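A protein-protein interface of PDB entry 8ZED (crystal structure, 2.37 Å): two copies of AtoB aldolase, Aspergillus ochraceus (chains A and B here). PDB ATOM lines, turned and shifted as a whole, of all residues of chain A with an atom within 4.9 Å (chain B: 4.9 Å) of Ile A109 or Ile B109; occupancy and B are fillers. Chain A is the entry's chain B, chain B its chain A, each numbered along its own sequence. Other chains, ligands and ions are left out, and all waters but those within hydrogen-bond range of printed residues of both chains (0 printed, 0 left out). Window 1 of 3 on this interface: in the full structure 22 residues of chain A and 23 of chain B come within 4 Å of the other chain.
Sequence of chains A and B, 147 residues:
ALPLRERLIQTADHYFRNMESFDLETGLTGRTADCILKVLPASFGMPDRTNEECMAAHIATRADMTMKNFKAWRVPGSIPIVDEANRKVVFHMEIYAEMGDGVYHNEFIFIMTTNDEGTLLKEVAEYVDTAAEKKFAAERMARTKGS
OH of Tyr B127 sits at hydrogen-bond distance from O of Glu A107 (2.7 Å).
The side-chain hydroxyl (OH) of Tyr A127 lies within hydrogen-bond range of the backbone carbonyl oxygen (O) of Glu B107 (2.5 Å).
The backbone carbonyl oxygen of Ile A109 sits at hydrogen-bond distance from the backbone NH of Tyr A127.
The backbone carbonyl oxygen (O) of Ile B109 lies within hydrogen-bond range of the backbone NH (N) of Tyr B127, 2.8 Å away.
A ring nitrogen (NE2) of His B92 lies within hydrogen-bond range of the side-chain carboxylate of Glu B107, 2.4 Å away.
The backbone NH of Leu A40 is in hydrogen-bond range of the backbone carbonyl oxygen of Glu A126 (2.7 Å).
The backbone carbonyl oxygen of Glu B126 is in hydrogen-bond range of the backbone NH of Leu B40, 2.8 Å away.
Among the printed residues, merely in contact across the chains: Leu A40 with His B92 (3.99 Å), His A92 with Leu B40 (3.9 Å), Glu A107 with Leu B40 (3.9 Å), Ile A109 with Ile B109 (3.9 Å), Ile A109 with Tyr B127 (3.5 Å), Tyr A127 with Ile B109 (3.6 Å) and Tyr A127 with Tyr B127 (3.3 Å).
Of the printed residues of chain B, His A92 touches Leu B40 (3.9 Å).
Of the printed residues of chain B, Glu A107 touches Leu B40 (3.9 Å) and Tyr B127 (2.7 Å).
Printed residues of chain B within 4 Å of Ile A109: Ile B109 and Tyr B127.
Phe A110 touches none of the printed residues of chain B.
Glu A126 touches none of the printed residues of chain B.
Of the printed residues of chain B, Tyr A127 touches Glu B107 (2.5 Å), Ile B109 (3.6 Å) and Tyr B127 (3.3 Å).
Of the printed residues of chain A, His B92 touches Leu A40 (3.99 Å).
Of the printed residues of chain A, Ile B109 touches Ile A109 and Tyr A127.
Printed residues of chain A within 4 Å of Tyr B127: Glu A107 (2.7 Å), Ile A109 (3.5 Å) and Tyr A127 (3.3 Å).
The nearest residue of chain B that does not touch Ile A109 is Ile B111 (4.2 Å).
The nearest printed residue of chain B that does not touch His A92 is Tyr B127 (5.4 Å).
Of the 12 printed residues of chain B, 5 touch a printed residue of chain A.
Of the 12 printed residues of chain A, 5 touch a printed residue of chain B.
Hydrophobic or aromatic side chains of chain A that line the printed part of chain B: Leu A40, His A92, Ile A109 and Tyr A127.
Among the printed residues, 9 pairs touch across the chains.
Leu A40 touches His B92, and with the chains exchanged His A92 touches Leu B40.
Glu A107 touches Leu B40, but with the chains exchanged Leu A40 does not touch Glu B107 (4.2 Å).
Ile A109 touches Tyr B127, and with the chains exchanged Tyr A127 touches Ile B109.
Tyr B127 touches its own counterpart, Tyr A127.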
ATOM      1  N   LEU A  40     -10.169  17.694   2.728  1.00  0.00           N
ATOM      2  CA  LEU A  40      -8.916  17.101   2.297  1.00  0.00           C
ATOM      3  C   LEU A  40      -7.777  18.105   2.436  1.00  0.00           C
ATOM      4  O   LEU A  40      -7.990  19.315   2.310  1.00  0.00           O
ATOM      5  CB  LEU A  40      -9.011  16.638   0.839  1.00  0.00           C
ATOM      6  CG  LEU A  40     -10.247  15.818   0.458  1.00  0.00           C
ATOM      7  CD1 LEU A  40     -10.151  15.337  -0.982  1.00  0.00           C
ATOM      8  CD2 LEU A  40     -10.445  14.647   1.407  1.00  0.00           C
ATOM      9  N   VAL A  90     -16.743  18.125 -10.426  1.00  0.00           N
ATOM     10  CA  VAL A  90     -15.508  18.687  -9.889  1.00  0.00           C
ATOM     11  C   VAL A  90     -15.428  20.157 -10.278  1.00  0.00           C
ATOM     12  O   VAL A  90     -15.705  20.524 -11.426  1.00  0.00           O
ATOM     13  CB  VAL A  90     -14.272  17.919 -10.393  1.00  0.00           C
ATOM     14  CG1 VAL A  90     -13.012  18.426  -9.704  1.00  0.00           C
ATOM     15  CG2 VAL A  90     -14.446  16.424 -10.170  1.00  0.00           C
ATOM     16  N   PHE A  91     -15.042  20.997  -9.317  1.00  0.00           N
ATOM     17  CA  PHE A  91     -14.914  22.430  -9.533  1.00  0.00           C
ATOM     18  C   PHE A  91     -13.520  22.900  -9.144  1.00  0.00           C
ATOM     19  O   PHE A  91     -12.827  22.275  -8.337  1.00  0.00           O
ATOM     20  CB  PHE A  91     -15.949  23.228  -8.726  1.00  0.00           C
ATOM     21  CG  PHE A  91     -17.359  23.065  -9.205  1.00  0.00           C
ATOM     22  CD1 PHE A  91     -17.749  23.562 -10.438  1.00  0.00           C
ATOM     23  CD2 PHE A  91     -18.306  22.441  -8.409  1.00  0.00           C
ATOM     24  CE1 PHE A  91     -19.053  23.423 -10.877  1.00  0.00           C
ATOM     25  CE2 PHE A  91     -19.610  22.301  -8.841  1.00  0.00           C
ATOM     26  CZ  PHE A  91     -19.983  22.793 -10.077  1.00  0.00           C
ATOM     27  N   HIS A  92     -13.122  24.026  -9.735  1.00  0.00           N
ATOM     28  CA  HIS A  92     -11.934  24.775  -9.333  1.00  0.00           C
ATOM     29  C   HIS A  92     -12.422  26.134  -8.851  1.00  0.00           C
ATOM     30  O   HIS A  92     -12.851  26.964  -9.659  1.00  0.00           O
ATOM     31  CB  HIS A  92     -10.945  24.908 -10.490  1.00  0.00           C
ATOM     32  CG  HIS A  92      -9.593  25.402 -10.075  1.00  0.00           C
ATOM     33  ND1 HIS A  92      -8.613  25.738 -10.985  1.00  0.00           N
ATOM     34  CD2 HIS A  92      -9.056  25.611  -8.850  1.00  0.00           C
ATOM     35  CE1 HIS A  92      -7.532  26.136 -10.339  1.00  0.00           C
ATOM     36  NE2 HIS A  92      -7.774  26.069  -9.042  1.00  0.00           N
ATOM     37  N   GLU A 107      -8.024  29.335  -2.500  1.00  0.00           N
ATOM     38  CA  GLU A 107      -8.345  28.569  -3.695  1.00  0.00           C
ATOM     39  C   GLU A 107      -8.611  27.119  -3.311  1.00  0.00           C
ATOM     40  O   GLU A 107      -7.949  26.572  -2.424  1.00  0.00           O
ATOM     41  CB  GLU A 107      -7.194  28.659  -4.702  1.00  0.00           C
ATOM     42  CG  GLU A 107      -7.389  27.909  -6.004  1.00  0.00           C
ATOM     43  CD  GLU A 107      -6.166  28.008  -6.896  1.00  0.00           C
ATOM     44  OE1 GLU A 107      -5.278  28.830  -6.591  1.00  0.00           O
ATOM     45  OE2 GLU A 107      -6.087  27.263  -7.896  1.00  0.00           O
ATOM     46  N   PHE A 108      -9.582  26.497  -3.978  1.00  0.00           N
ATOM     47  CA  PHE A 108     -10.049  25.175  -3.587  1.00  0.00           C
ATOM     48  C   PHE A 108     -10.218  24.277  -4.804  1.00  0.00           C
ATOM     49  O   PHE A 108     -10.322  24.740  -5.944  1.00  0.00           O
ATOM     50  CB  PHE A 108     -11.387  25.242  -2.837  1.00  0.00           C
ATOM     51  CG  PHE A 108     -11.325  25.991  -1.540  1.00  0.00           C
ATOM     52  CD1 PHE A 108     -11.504  27.363  -1.507  1.00  0.00           C
ATOM     53  CD2 PHE A 108     -11.106  25.318  -0.349  1.00  0.00           C
ATOM     54  CE1 PHE A 108     -11.455  28.053  -0.311  1.00  0.00           C
ATOM     55  CE2 PHE A 108     -11.057  26.004   0.850  1.00  0.00           C
ATOM     56  CZ  PHE A 108     -11.231  27.372   0.868  1.00  0.00           C
ATOM     57  N   ILE A 109     -10.248  22.974  -4.534  1.00  0.00           N
ATOM     58  CA  ILE A 109     -10.716  21.963  -5.473  1.00  0.00           C
ATOM     59  C   ILE A 109     -11.897  21.263  -4.814  1.00  0.00           C
ATOM     60  O   ILE A 109     -11.748  20.667  -3.739  1.00  0.00           O
ATOM     61  CB  ILE A 109      -9.614  20.958  -5.843  1.00  0.00           C
ATOM     62  CG1 ILE A 109      -8.627  21.584  -6.831  1.00  0.00           C
ATOM     63  CG2 ILE A 109     -10.220  19.690  -6.428  1.00  0.00           C
ATOM     64  CD1 ILE A 109      -9.242  21.943  -8.165  1.00  0.00           C
ATOM     65  N   PHE A 110     -13.065  21.350  -5.440  1.00  0.00           N
ATOM     66  CA  PHE A 110     -14.295  20.809  -4.881  1.00  0.00           C
ATOM     67  C   PHE A 110     -14.736  19.576  -5.657  1.00  0.00           C
ATOM     68  O   PHE A 110     -14.658  19.543  -6.888  1.00  0.00           O
ATOM     69  CB  PHE A 110     -15.414  21.855  -4.893  1.00  0.00           C
ATOM     70  CG  PHE A 110     -15.446  22.722  -3.666  1.00  0.00           C
ATOM     71  CD1 PHE A 110     -16.127  22.311  -2.533  1.00  0.00           C
ATOM     72  CD2 PHE A 110     -14.798  23.944  -3.646  1.00  0.00           C
ATOM     73  CE1 PHE A 110     -16.163  23.104  -1.402  1.00  0.00           C
ATOM     74  CE2 PHE A 110     -14.830  24.742  -2.518  1.00  0.00           C
ATOM     75  CZ  PHE A 110     -15.512  24.320  -1.394  1.00  0.00           C
ATOM     76  N   ILE A 111     -15.201  18.564  -4.926  1.00  0.00           N
ATOM     77  CA  ILE A 111     -15.733  17.338  -5.509  1.00  0.00           C
ATOM     78  C   ILE A 111     -17.095  17.080  -4.884  1.00  0.00           C
ATOM     79  O   ILE A 111     -17.197  16.898  -3.664  1.00  0.00           O
ATOM     80  CB  ILE A 111     -14.800  16.135  -5.287  1.00  0.00           C
ATOM     81  CG1 ILE A 111     -13.436  16.386  -5.932  1.00  0.00           C
ATOM     82  CG2 ILE A 111     -15.431  14.867  -5.841  1.00  0.00           C
ATOM     83  CD1 ILE A 111     -12.464  15.239  -5.763  1.00  0.00           C
ATOM     84  N   ALA A 125     -16.571  17.061  -0.918  1.00  0.00           N
ATOM     85  CA  ALA A 125     -15.174  16.938  -0.525  1.00  0.00           C
ATOM     86  C   ALA A 125     -14.397  18.129  -1.066  1.00  0.00           C
ATOM     87  O   ALA A 125     -14.511  18.459  -2.251  1.00  0.00           O
ATOM     88  CB  ALA A 125     -14.569  15.628  -1.037  1.00  0.00           C
ATOM     89  N   GLU A 126     -13.607  18.767  -0.205  1.00  0.00           N
ATOM     90  CA  GLU A 126     -12.851  19.958  -0.573  1.00  0.00           C
ATOM     91  C   GLU A 126     -11.407  19.821  -0.112  1.00  0.00           C
ATOM     92  O   GLU A 126     -11.150  19.538   1.063  1.00  0.00           O
ATOM     93  CB  GLU A 126     -13.482  21.221   0.030  1.00  0.00           C
ATOM     94  CG  GLU A 126     -14.155  20.996   1.377  1.00  0.00           C
ATOM     95  CD  GLU A 126     -14.652  22.282   2.015  1.00  0.00           C
ATOM     96  OE1 GLU A 126     -13.867  23.249   2.106  1.00  0.00           O
ATOM     97  OE2 GLU A 126     -15.831  22.326   2.427  1.00  0.00           O
ATOM     98  N   TYR A 127     -10.474  20.018  -1.040  1.00  0.00           N
ATOM     99  CA  TYR A 127      -9.049  20.086  -0.737  1.00  0.00           C
ATOM    100  C   TYR A 127      -8.670  21.548  -0.529  1.00  0.00           C
ATOM    101  O   TYR A 127      -8.937  22.390  -1.395  1.00  0.00           O
ATOM    102  CB  TYR A 127      -8.222  19.468  -1.867  1.00  0.00           C
ATOM    103  CG  TYR A 127      -6.843  18.994  -1.458  1.00  0.00           C
ATOM    104  CD1 TYR A 127      -5.901  19.881  -0.954  1.00  0.00           C
ATOM    105  CD2 TYR A 127      -6.479  17.661  -1.591  1.00  0.00           C
ATOM    106  CE1 TYR A 127      -4.640  19.454  -0.585  1.00  0.00           C
ATOM    107  CE2 TYR A 127      -5.220  17.223  -1.224  1.00  0.00           C
ATOM    108  CZ  TYR A 127      -4.304  18.125  -0.722  1.00  0.00           C
ATOM    109  OH  TYR A 127      -3.048  17.702  -0.353  1.00  0.00           O
ATOM    110  N   LEU B  40      -1.116  23.474  -8.227  1.00  0.00           N
ATOM    111  CA  LEU B  40      -2.142  24.182  -7.482  1.00  0.00           C
ATOM    112  C   LEU B  40      -1.874  24.093  -5.984  1.00  0.00           C
ATOM    113  O   LEU B  40      -1.310  23.102  -5.506  1.00  0.00           O
ATOM    114  CB  LEU B  40      -3.525  23.600  -7.784  1.00  0.00           C
ATOM    115  CG  LEU B  40      -3.919  23.470  -9.256  1.00  0.00           C
ATOM    116  CD1 LEU B  40      -5.315  22.875  -9.384  1.00  0.00           C
ATOM    117  CD2 LEU B  40      -3.838  24.816  -9.960  1.00  0.00           C
ATOM    118  N   VAL B  90      -9.915  12.716 -13.130  1.00  0.00           N
ATOM    119  CA  VAL B  90      -9.583  13.242 -11.809  1.00  0.00           C
ATOM    120  C   VAL B  90      -9.195  12.079 -10.906  1.00  0.00           C
ATOM    121  O   VAL B  90      -9.891  11.058 -10.865  1.00  0.00           O
ATOM    122  CB  VAL B  90     -10.753  14.040 -11.209  1.00  0.00           C
ATOM    123  CG1 VAL B  90     -10.347  14.665  -9.882  1.00  0.00           C
ATOM    124  CG2 VAL B  90     -11.226  15.106 -12.186  1.00  0.00           C
ATOM    125  N   PHE B  91      -8.090  12.240 -10.179  1.00  0.00           N
ATOM    126  CA  PHE B  91      -7.569  11.208  -9.294  1.00  0.00           C
ATOM    127  C   PHE B  91      -7.369  11.766  -7.892  1.00  0.00           C
ATOM    128  O   PHE B  91      -7.025  12.938  -7.713  1.00  0.00           O
ATOM    129  CB  PHE B  91      -6.231  10.649  -9.804  1.00  0.00           C
ATOM    130  CG  PHE B  91      -6.363   9.689 -10.951  1.00  0.00           C
ATOM    131  CD1 PHE B  91      -7.408   8.783 -11.002  1.00  0.00           C
ATOM    132  CD2 PHE B  91      -5.431   9.689 -11.977  1.00  0.00           C
ATOM    133  CE1 PHE B  91      -7.523   7.897 -12.058  1.00  0.00           C
ATOM    134  CE2 PHE B  91      -5.542   8.807 -13.035  1.00  0.00           C
ATOM    135  CZ  PHE B  91      -6.589   7.910 -13.076  1.00  0.00           C
ATOM    136  N   HIS B  92      -7.586  10.907  -6.897  1.00  0.00           N
ATOM    137  CA  HIS B  92      -7.237  11.181  -5.507  1.00  0.00           C
ATOM    138  C   HIS B  92      -6.074  10.260  -5.156  1.00  0.00           C
ATOM    139  O   HIS B  92      -6.263   9.051  -4.988  1.00  0.00           O
ATOM    140  CB  HIS B  92      -8.432  10.957  -4.582  1.00  0.00           C
ATOM    141  CG  HIS B  92      -8.208  11.431  -3.180  1.00  0.00           C
ATOM    142  ND1 HIS B  92      -9.018  11.056  -2.130  1.00  0.00           N
ATOM    143  CD2 HIS B  92      -7.268  12.253  -2.655  1.00  0.00           C
ATOM    144  CE1 HIS B  92      -8.584  11.625  -1.018  1.00  0.00           C
ATOM    145  NE2 HIS B  92      -7.525  12.356  -1.309  1.00  0.00           N
ATOM    146  N   GLU B 107      -0.570  13.734   0.078  1.00  0.00           N
ATOM    147  CA  GLU B 107      -1.851  13.437  -0.546  1.00  0.00           C
ATOM    148  C   GLU B 107      -2.161  14.507  -1.583  1.00  0.00           C
ATOM    149  O   GLU B 107      -1.971  15.701  -1.330  1.00  0.00           O
ATOM    150  CB  GLU B 107      -2.959  13.371   0.513  1.00  0.00           C
ATOM    151  CG  GLU B 107      -4.355  13.103  -0.020  1.00  0.00           C
ATOM    152  CD  GLU B 107      -5.381  13.026   1.095  1.00  0.00           C
ATOM    153  OE1 GLU B 107      -4.973  12.854   2.263  1.00  0.00           O
ATOM    154  OE2 GLU B 107      -6.591  13.145   0.807  1.00  0.00           O
ATOM    155  N   PHE B 108      -2.636  14.078  -2.753  1.00  0.00           N
ATOM    156  CA  PHE B 108      -2.777  14.965  -3.898  1.00  0.00           C
ATOM    157  C   PHE B 108      -4.128  14.771  -4.572  1.00  0.00           C
ATOM    158  O   PHE B 108      -4.799  13.749  -4.400  1.00  0.00           O
ATOM    159  CB  PHE B 108      -1.668  14.728  -4.936  1.00  0.00           C
ATOM    160  CG  PHE B 108      -0.275  14.894  -4.397  1.00  0.00           C
ATOM    161  CD1 PHE B 108       0.340  13.868  -3.700  1.00  0.00           C
ATOM    162  CD2 PHE B 108       0.426  16.069  -4.607  1.00  0.00           C
ATOM    163  CE1 PHE B 108       1.622  14.016  -3.207  1.00  0.00           C
ATOM    164  CE2 PHE B 108       1.710  16.222  -4.119  1.00  0.00           C
ATOM    165  CZ  PHE B 108       2.308  15.194  -3.418  1.00  0.00           C
ATOM    166  N   ILE B 109      -4.512  15.780  -5.350  1.00  0.00           N
ATOM    167  CA  ILE B 109      -5.620  15.700  -6.296  1.00  0.00           C
ATOM    168  C   ILE B 109      -5.048  15.990  -7.677  1.00  0.00           C
ATOM    169  O   ILE B 109      -4.450  17.051  -7.893  1.00  0.00           O
ATOM    170  CB  ILE B 109      -6.748  16.684  -5.953  1.00  0.00           C
ATOM    171  CG1 ILE B 109      -7.488  16.234  -4.691  1.00  0.00           C
ATOM    172  CG2 ILE B 109      -7.712  16.821  -7.124  1.00  0.00           C
ATOM    173  CD1 ILE B 109      -8.207  14.912  -4.843  1.00  0.00           C
ATOM    174  N   PHE B 110      -5.220  15.051  -8.603  1.00  0.00           N
ATOM    175  CA  PHE B 110      -4.659  15.161  -9.942  1.00  0.00           C
ATOM    176  C   PHE B 110      -5.766  15.341 -10.972  1.00  0.00           C
ATOM    177  O   PHE B 110      -6.809  14.684 -10.902  1.00  0.00           O
ATOM    178  CB  PHE B 110      -3.822  13.927 -10.291  1.00  0.00           C
ATOM    179  CG  PHE B 110      -2.395  14.010  -9.824  1.00  0.00           C
ATOM    180  CD1 PHE B 110      -2.035  13.564  -8.563  1.00  0.00           C
ATOM    181  CD2 PHE B 110      -1.415  14.533 -10.650  1.00  0.00           C
ATOM    182  CE1 PHE B 110      -0.722  13.639  -8.136  1.00  0.00           C
ATOM    183  CE2 PHE B 110      -0.100  14.612 -10.229  1.00  0.00           C
ATOM    184  CZ  PHE B 110       0.246  14.164  -8.969  1.00  0.00           C
ATOM    185  N   ILE B 111      -5.529  16.239 -11.927  1.00  0.00           N
ATOM    186  CA  ILE B 111      -6.448  16.493 -13.031  1.00  0.00           C
ATOM    187  C   ILE B 111      -5.663  16.350 -14.326  1.00  0.00           C
ATOM    188  O   ILE B 111      -4.725  17.118 -14.574  1.00  0.00           O
ATOM    189  CB  ILE B 111      -7.094  17.886 -12.941  1.00  0.00           C
ATOM    190  CG1 ILE B 111      -7.786  18.072 -11.589  1.00  0.00           C
ATOM    191  CG2 ILE B 111      -8.083  18.086 -14.081  1.00  0.00           C
ATOM    192  CD1 ILE B 111      -8.391  19.444 -11.399  1.00  0.00           C
ATOM    193  N   ALA B 125      -2.520  18.720 -13.958  1.00  0.00           N
ATOM    194  CA  ALA B 125      -2.695  19.670 -12.869  1.00  0.00           C
ATOM    195  C   ALA B 125      -2.812  18.911 -11.556  1.00  0.00           C
ATOM    196  O   ALA B 125      -3.549  17.924 -11.471  1.00  0.00           O
ATOM    197  CB  ALA B 125      -3.933  20.545 -13.091  1.00  0.00           C
ATOM    198  N   GLU B 126      -2.092  19.375 -10.537  1.00  0.00           N
ATOM    199  CA  GLU B 126      -2.054  18.714  -9.239  1.00  0.00           C
ATOM    200  C   GLU B 126      -2.217  19.744  -8.132  1.00  0.00           C
ATOM    201  O   GLU B 126      -1.497  20.746  -8.101  1.00  0.00           O
ATOM    202  CB  GLU B 126      -0.743  17.942  -9.055  1.00  0.00           C
ATOM    203  CG  GLU B 126       0.494  18.706  -9.506  1.00  0.00           C
ATOM    204  CD  GLU B 126       1.783  17.965  -9.211  1.00  0.00           C
ATOM    205  OE1 GLU B 126       1.895  17.377  -8.115  1.00  0.00           O
ATOM    206  OE2 GLU B 126       2.681  17.964 -10.078  1.00  0.00           O
ATOM    207  N   TYR B 127      -3.164  19.497  -7.229  1.00  0.00           N
ATOM    208  CA  TYR B 127      -3.299  20.308  -6.027  1.00  0.00           C
ATOM    209  C   TYR B 127      -2.434  19.711  -4.926  1.00  0.00           C
ATOM    210  O   TYR B 127      -2.440  18.497  -4.701  1.00  0.00           O
ATOM    211  CB  TYR B 127      -4.756  20.392  -5.571  1.00  0.00           C
ATOM    212  CG  TYR B 127      -5.044  21.604  -4.708  1.00  0.00           C
ATOM    213  CD1 TYR B 127      -4.576  21.681  -3.402  1.00  0.00           C
ATOM    214  CD2 TYR B 127      -5.781  22.672  -5.200  1.00  0.00           C
ATOM    215  CE1 TYR B 127      -4.835  22.785  -2.612  1.00  0.00           C
ATOM    216  CE2 TYR B 127      -6.046  23.781  -4.416  1.00  0.00           C
ATOM    217  CZ  TYR B 127      -5.571  23.831  -3.124  1.00  0.00           C
ATOM    218  OH  TYR B 127      -5.830  24.932  -2.339  1.00  0.00           O
